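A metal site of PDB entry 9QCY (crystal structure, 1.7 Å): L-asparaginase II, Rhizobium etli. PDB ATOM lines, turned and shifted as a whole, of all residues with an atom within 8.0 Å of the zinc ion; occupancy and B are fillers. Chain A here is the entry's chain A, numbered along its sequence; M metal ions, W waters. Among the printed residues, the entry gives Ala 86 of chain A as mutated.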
ATOM      1  N   ARG A  53      13.461   3.318  27.147  1.00  0.00           N
ATOM      2  CA  ARG A  53      13.242   1.845  27.204  1.00  0.00           C
ATOM      3  C   ARG A  53      14.274   1.132  26.326  1.00  0.00           C
ATOM      4  O   ARG A  53      15.452   1.478  26.417  1.00  0.00           O
ATOM      5  CB  ARG A  53      11.763   1.565  26.885  1.00  0.00           C
ATOM      6  CG  ARG A  53      10.780   2.342  27.786  1.00  0.00           C
ATOM      7  CD  ARG A  53      10.752   1.869  29.267  1.00  0.00           C
ATOM      8  NE  ARG A  53      10.341   0.471  29.325  1.00  0.00           N
ATOM      9  CZ  ARG A  53       9.095   0.059  29.152  1.00  0.00           C
ATOM     10  NH1 ARG A  53       8.099   0.902  28.923  1.00  0.00           N
ATOM     11  NH2 ARG A  53       8.838  -1.247  29.177  1.00  0.00           N
ATOM     12  N   SER A  54      13.880   0.141  25.501  1.00  0.00           N
ATOM     13  CA  SER A  54      14.860  -0.557  24.673  1.00  0.00           C
ATOM     14  C   SER A  54      15.574   0.361  23.692  1.00  0.00           C
ATOM     15  O   SER A  54      16.661   0.001  23.228  1.00  0.00           O
ATOM     16  CB  SER A  54      14.199  -1.700  23.892  1.00  0.00           C
ATOM     17  OG  SER A  54      13.985  -2.836  24.713  1.00  0.00           O
ATOM     18  N   LYS A  57      19.216   1.026  24.352  1.00  0.00           N
ATOM     19  CA  LYS A  57      20.180  -0.059  24.443  1.00  0.00           C
ATOM     20  C   LYS A  57      21.514   0.214  23.748  1.00  0.00           C
ATOM     21  O   LYS A  57      22.515  -0.339  24.219  1.00  0.00           O
ATOM     22  CB  LYS A  57      19.571  -1.360  23.932  1.00  0.00           C
ATOM     23  CG  LYS A  57      18.648  -2.024  24.930  1.00  0.00           C
ATOM     24  CD  LYS A  57      18.030  -3.285  24.311  1.00  0.00           C
ATOM     25  CE  LYS A  57      17.159  -3.994  25.323  1.00  0.00           C
ATOM     26  NZ  LYS A  57      15.969  -4.690  24.674  1.00  0.00           N
ATOM     27  N   GLN A  60      23.599   1.724  26.456  1.00  0.00           N
ATOM     28  CA  GLN A  60      23.972   0.665  27.384  1.00  0.00           C
ATOM     29  C   GLN A  60      25.050  -0.226  26.781  1.00  0.00           C
ATOM     30  O   GLN A  60      25.997  -0.615  27.483  1.00  0.00           O
ATOM     31  CB  GLN A  60      22.746  -0.140  27.779  1.00  0.00           C
ATOM     32  CG  GLN A  60      21.872   0.656  28.710  1.00  0.00           C
ATOM     33  CD  GLN A  60      20.434   0.207  28.744  1.00  0.00           C
ATOM     34  OE1 GLN A  60      19.819  -0.018  27.679  1.00  0.00           O
ATOM     35  NE2 GLN A  60      19.889   0.055  29.956  1.00  0.00           N
ATOM     36  N   ALA A  85      19.538  -5.320  21.156  1.00  0.00           N
ATOM     37  CA  ALA A  85      18.310  -5.889  20.604  1.00  0.00           C
ATOM     38  C   ALA A  85      17.146  -5.819  21.566  1.00  0.00           C
ATOM     39  O   ALA A  85      17.311  -5.964  22.773  1.00  0.00           O
ATOM     40  CB  ALA A  85      18.518  -7.365  20.243  1.00  0.00           C
ATOM     41  N   ALA A  86      15.936  -5.704  21.000  1.00  0.00           N
ATOM     42  CA  ALA A  86      14.715  -6.209  21.636  1.00  0.00           C
ATOM     43  C   ALA A  86      14.227  -7.408  20.829  1.00  0.00           C
ATOM     44  O   ALA A  86      13.285  -7.321  20.066  1.00  0.00           O
ATOM     45  CB  ALA A  86      13.633  -5.125  21.720  1.00  0.00           C
ATOM     46  N   CYS A 113      17.309 -10.739  34.564  1.00  0.00           N
ATOM     47  CA  CYS A 113      16.104 -10.462  33.773  1.00  0.00           C
ATOM     48  C   CYS A 113      15.188 -11.671  33.798  1.00  0.00           C
ATOM     49  O   CYS A 113      15.598 -12.793  34.116  1.00  0.00           O
ATOM     50  CB  CYS A 113      16.473 -10.112  32.332  1.00  0.00           C
ATOM     51  SG  CYS A 113      17.578 -11.331  31.527  1.00  0.00           S
ATOM     52  N   SER A 139      14.568 -13.652  27.606  1.00  0.00           N
ATOM     53  CA  SER A 139      14.243 -12.234  27.670  1.00  0.00           C
ATOM     54  C   SER A 139      14.678 -11.528  26.409  1.00  0.00           C
ATOM     55  O   SER A 139      15.760 -11.788  25.868  1.00  0.00           O
ATOM     56  CB  SER A 139      14.932 -11.572  28.868  1.00  0.00           C
ATOM     57  OG  SER A 139      14.904 -10.169  28.724  1.00  0.00           O
ATOM     58  N   ASN A 140      13.828 -10.612  25.931  1.00  0.00           N
ATOM     59  CA  ASN A 140      14.189  -9.773  24.805  1.00  0.00           C
ATOM     60  C   ASN A 140      15.438  -8.950  25.079  1.00  0.00           C
ATOM     61  O   ASN A 140      16.130  -8.547  24.143  1.00  0.00           O
ATOM     62  CB  ASN A 140      13.003  -8.874  24.428  1.00  0.00           C
ATOM     63  CG  ASN A 140      12.922  -7.642  25.281  1.00  0.00           C
ATOM     64  OD1 ASN A 140      13.448  -6.573  24.919  1.00  0.00           O
ATOM     65  ND2 ASN A 140      12.291  -7.771  26.431  1.00  0.00           N
ATOM     66  N   CYS A 141      15.755  -8.701  26.351  1.00  0.00           N
ATOM     67  CA  CYS A 141      16.950  -7.963  26.744  1.00  0.00           C
ATOM     68  C   CYS A 141      18.119  -8.873  27.097  1.00  0.00           C
ATOM     69  O   CYS A 141      19.112  -8.404  27.692  1.00  0.00           O
ATOM     70  CB  CYS A 141      16.636  -7.033  27.937  1.00  0.00           C
ATOM     71  SG  CYS A 141      15.257  -5.850  27.687  1.00  0.00           S
ATOM     72  N   SER A 142      18.041 -10.162  26.777  1.00  0.00           N
ATOM     73  CA  SER A 142      19.016 -11.108  27.301  1.00  0.00           C
ATOM     74  C   SER A 142      20.439 -10.729  26.921  1.00  0.00           C
ATOM     75  O   SER A 142      21.353 -10.849  27.744  1.00  0.00           O
ATOM     76  CB  SER A 142      18.699 -12.516  26.816  1.00  0.00           C
ATOM     77  OG  SER A 142      18.716 -12.556  25.396  1.00  0.00           O
ATOM     78  N   LYS A 144      21.669  -7.695  26.338  1.00  0.00           N
ATOM     79  CA  LYS A 144      22.097  -6.601  27.220  1.00  0.00           C
ATOM     80  C   LYS A 144      22.553  -7.144  28.569  1.00  0.00           C
ATOM     81  O   LYS A 144      23.606  -6.760  29.100  1.00  0.00           O
ATOM     82  CB  LYS A 144      20.951  -5.603  27.393  1.00  0.00           C
ATOM     83  CG  LYS A 144      21.235  -4.522  28.433  1.00  0.00           C
ATOM     84  CD  LYS A 144      20.055  -3.525  28.494  1.00  0.00           C
ATOM     85  CE  LYS A 144      18.720  -4.208  28.739  1.00  0.00           C
ATOM     86  NZ  LYS A 144      17.738  -3.207  29.165  1.00  0.00           N
ATOM     87  N   HIS A 145      21.755  -8.055  29.138  1.00  0.00           N
ATOM     88  CA  HIS A 145      22.095  -8.597  30.450  1.00  0.00           C
ATOM     89  C   HIS A 145      23.384  -9.415  30.421  1.00  0.00           C
ATOM     90  O   HIS A 145      24.178  -9.345  31.374  1.00  0.00           O
ATOM     91  CB  HIS A 145      20.925  -9.399  31.002  1.00  0.00           C
ATOM     92  CG  HIS A 145      19.853  -8.537  31.577  1.00  0.00           C
ATOM     93  ND1 HIS A 145      19.724  -8.325  32.934  1.00  0.00           N
ATOM     94  CD2 HIS A 145      18.866  -7.831  30.975  1.00  0.00           C
ATOM     95  CE1 HIS A 145      18.709  -7.506  33.145  1.00  0.00           C
ATOM     96  NE2 HIS A 145      18.160  -7.203  31.978  1.00  0.00           N
ATOM     97  N   MET A 148      26.167  -6.990  30.488  1.00  0.00           N
ATOM     98  CA  MET A 148      26.401  -6.386  31.791  1.00  0.00           C
ATOM     99  C   MET A 148      27.032  -7.364  32.772  1.00  0.00           C
ATOM    100  O   MET A 148      27.870  -6.959  33.586  1.00  0.00           O
ATOM    101  CB  MET A 148      25.114  -5.803  32.329  1.00  0.00           C
ATOM    102  CG  MET A 148      24.857  -4.436  31.759  1.00  0.00           C
ATOM    103  SD  MET A 148      23.222  -3.920  32.161  1.00  0.00           S
ATOM    104  CE  MET A 148      23.122  -2.397  31.216  1.00  0.00           C
ATOM    105  N   ASP A 193      13.101  -0.990  34.550  1.00  0.00           N
ATOM    106  CA  ASP A 193      12.582  -1.567  33.322  1.00  0.00           C
ATOM    107  C   ASP A 193      11.878  -2.910  33.532  1.00  0.00           C
ATOM    108  O   ASP A 193      11.959  -3.532  34.604  1.00  0.00           O
ATOM    109  CB  ASP A 193      13.732  -1.758  32.327  1.00  0.00           C
ATOM    110  CG  ASP A 193      13.526  -1.014  31.017  1.00  0.00           C
ATOM    111  OD1 ASP A 193      12.362  -0.736  30.682  1.00  0.00           O
ATOM    112  OD2 ASP A 193      14.526  -0.708  30.331  1.00  0.00           O
ATOM    113  N   GLY A 194      11.208  -3.410  32.461  1.00  0.00           N
ATOM    114  CA  GLY A 194      10.595  -4.725  32.528  1.00  0.00           C
ATOM    115  C   GLY A 194      11.590  -5.829  32.760  1.00  0.00           C
ATOM    116  O   GLY A 194      11.259  -6.883  33.300  1.00  0.00           O
ATOM    117  N   CYS A 195      12.834  -5.644  32.285  1.00  0.00           N
ATOM    118  CA  CYS A 195      13.906  -6.591  32.488  1.00  0.00           C
ATOM    119  C   CYS A 195      14.583  -6.423  33.847  1.00  0.00           C
ATOM    120  O   CYS A 195      15.568  -7.107  34.113  1.00  0.00           O
ATOM    121  CB  CYS A 195      14.947  -6.449  31.369  1.00  0.00           C
ATOM    122  SG  CYS A 195      15.766  -4.836  31.345  1.00  0.00           S
ATOM    123  N   ASN A 196      14.094  -5.495  34.671  1.00  0.00           N
ATOM    124  CA  ASN A 196      14.553  -5.214  36.036  1.00  0.00           C
ATOM    125  C   ASN A 196      15.901  -4.482  36.115  1.00  0.00           C
ATOM    126  O   ASN A 196      16.533  -4.467  37.179  1.00  0.00           O
ATOM    127  CB  ASN A 196      14.613  -6.499  36.872  1.00  0.00           C
ATOM    128  CG  ASN A 196      14.471  -6.248  38.349  1.00  0.00           C
ATOM    129  OD1 ASN A 196      13.723  -5.389  38.771  1.00  0.00           O
ATOM    130  ND2 ASN A 196      15.217  -7.005  39.158  1.00  0.00           N
ATOM    131  N   LEU A 197      16.384  -3.844  35.010  1.00  0.00           N
ATOM    132  CA  LEU A 197      17.487  -2.861  35.059  1.00  0.00           C
ATOM    133  C   LEU A 197      17.010  -1.427  35.272  1.00  0.00           C
ATOM    134  O   LEU A 197      15.885  -1.085  34.930  1.00  0.00           O
ATOM    135  CB  LEU A 197      18.319  -2.886  33.792  1.00  0.00           C
ATOM    136  CG  LEU A 197      19.045  -4.169  33.460  1.00  0.00           C
ATOM    137  CD1 LEU A 197      19.794  -4.030  32.135  1.00  0.00           C
ATOM    138  CD2 LEU A 197      20.176  -4.384  34.477  1.00  0.00           C
ATOM    139  N   PRO A 198      17.908  -0.553  35.754  1.00  0.00           N
ATOM    140  CA  PRO A 198      17.653   0.881  35.678  1.00  0.00           C
ATOM    141  C   PRO A 198      17.415   1.302  34.222  1.00  0.00           C
ATOM    142  O   PRO A 198      18.083   0.830  33.302  1.00  0.00           O
ATOM    143  CB  PRO A 198      18.939   1.505  36.247  1.00  0.00           C
ATOM    144  CG  PRO A 198      19.519   0.444  37.083  1.00  0.00           C
ATOM    145  CD  PRO A 198      19.240  -0.829  36.363  1.00  0.00           C
ATOM    146  N   THR A 199      16.441   2.207  34.011  1.00  0.00           N
ATOM    147  CA  THR A 199      16.109   2.629  32.663  1.00  0.00           C
ATOM    148  C   THR A 199      15.885   4.136  32.622  1.00  0.00           C
ATOM    149  O   THR A 199      15.269   4.702  33.536  1.00  0.00           O
ATOM    150  CB  THR A 199      14.881   1.859  32.122  1.00  0.00           C
ATOM    151  OG1 THR A 199      14.838   1.965  30.688  1.00  0.00           O
ATOM    152  CG2 THR A 199      13.542   2.318  32.744  1.00  0.00           C
HETATM  153 ZN    ZN M   1      15.802  -4.189  29.175  1.00  0.00          ZN
HETATM  154  O   HOH W   1      14.747  -2.625  28.414  1.00  0.00           O
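The backbone carbonyl oxygen (O) of Cys 195 sits close to a ring nitrogen (NE2) of His 145. NZ of Lys 57 lies close to SG of Cys 141. The side-chain sulfur of Cys 141 lies close to the side-chain amide oxygen of Asn 140 (3.4 Å). The side-chain hydroxyl (OG) of Ser 139 is in hydrogen-bond range of the backbone NH (N) of Cys 141 (2.9 Å). The side-chain carboxylate of Asp 193 lies within salt-bridge range of the guanidinium group of Arg 53 (2.7 Å). The side-chain hydroxyl of Thr 199 sits at hydrogen-bond distance from the side-chain carboxylate of Asp 193, at 2.7 Å.
Asp 193 touches the zinc ion. Within 4 Å of the zinc ion: Cys 141, Lys 144, Asp 193 and Cys 195. The nearest printed residue that does not touch the zinc ion is Lys 57 (4.1 Å).
Water W1 binds the zinc ion. NZ of Lys 144 is bound to the zinc ion (2.2 Å). SG of Cys 195 binds the zinc ion (2.3 Å). SG of Cys 141 is bound to the zinc ion (2.3 Å). The zinc ion has four donor atoms within binding distance.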
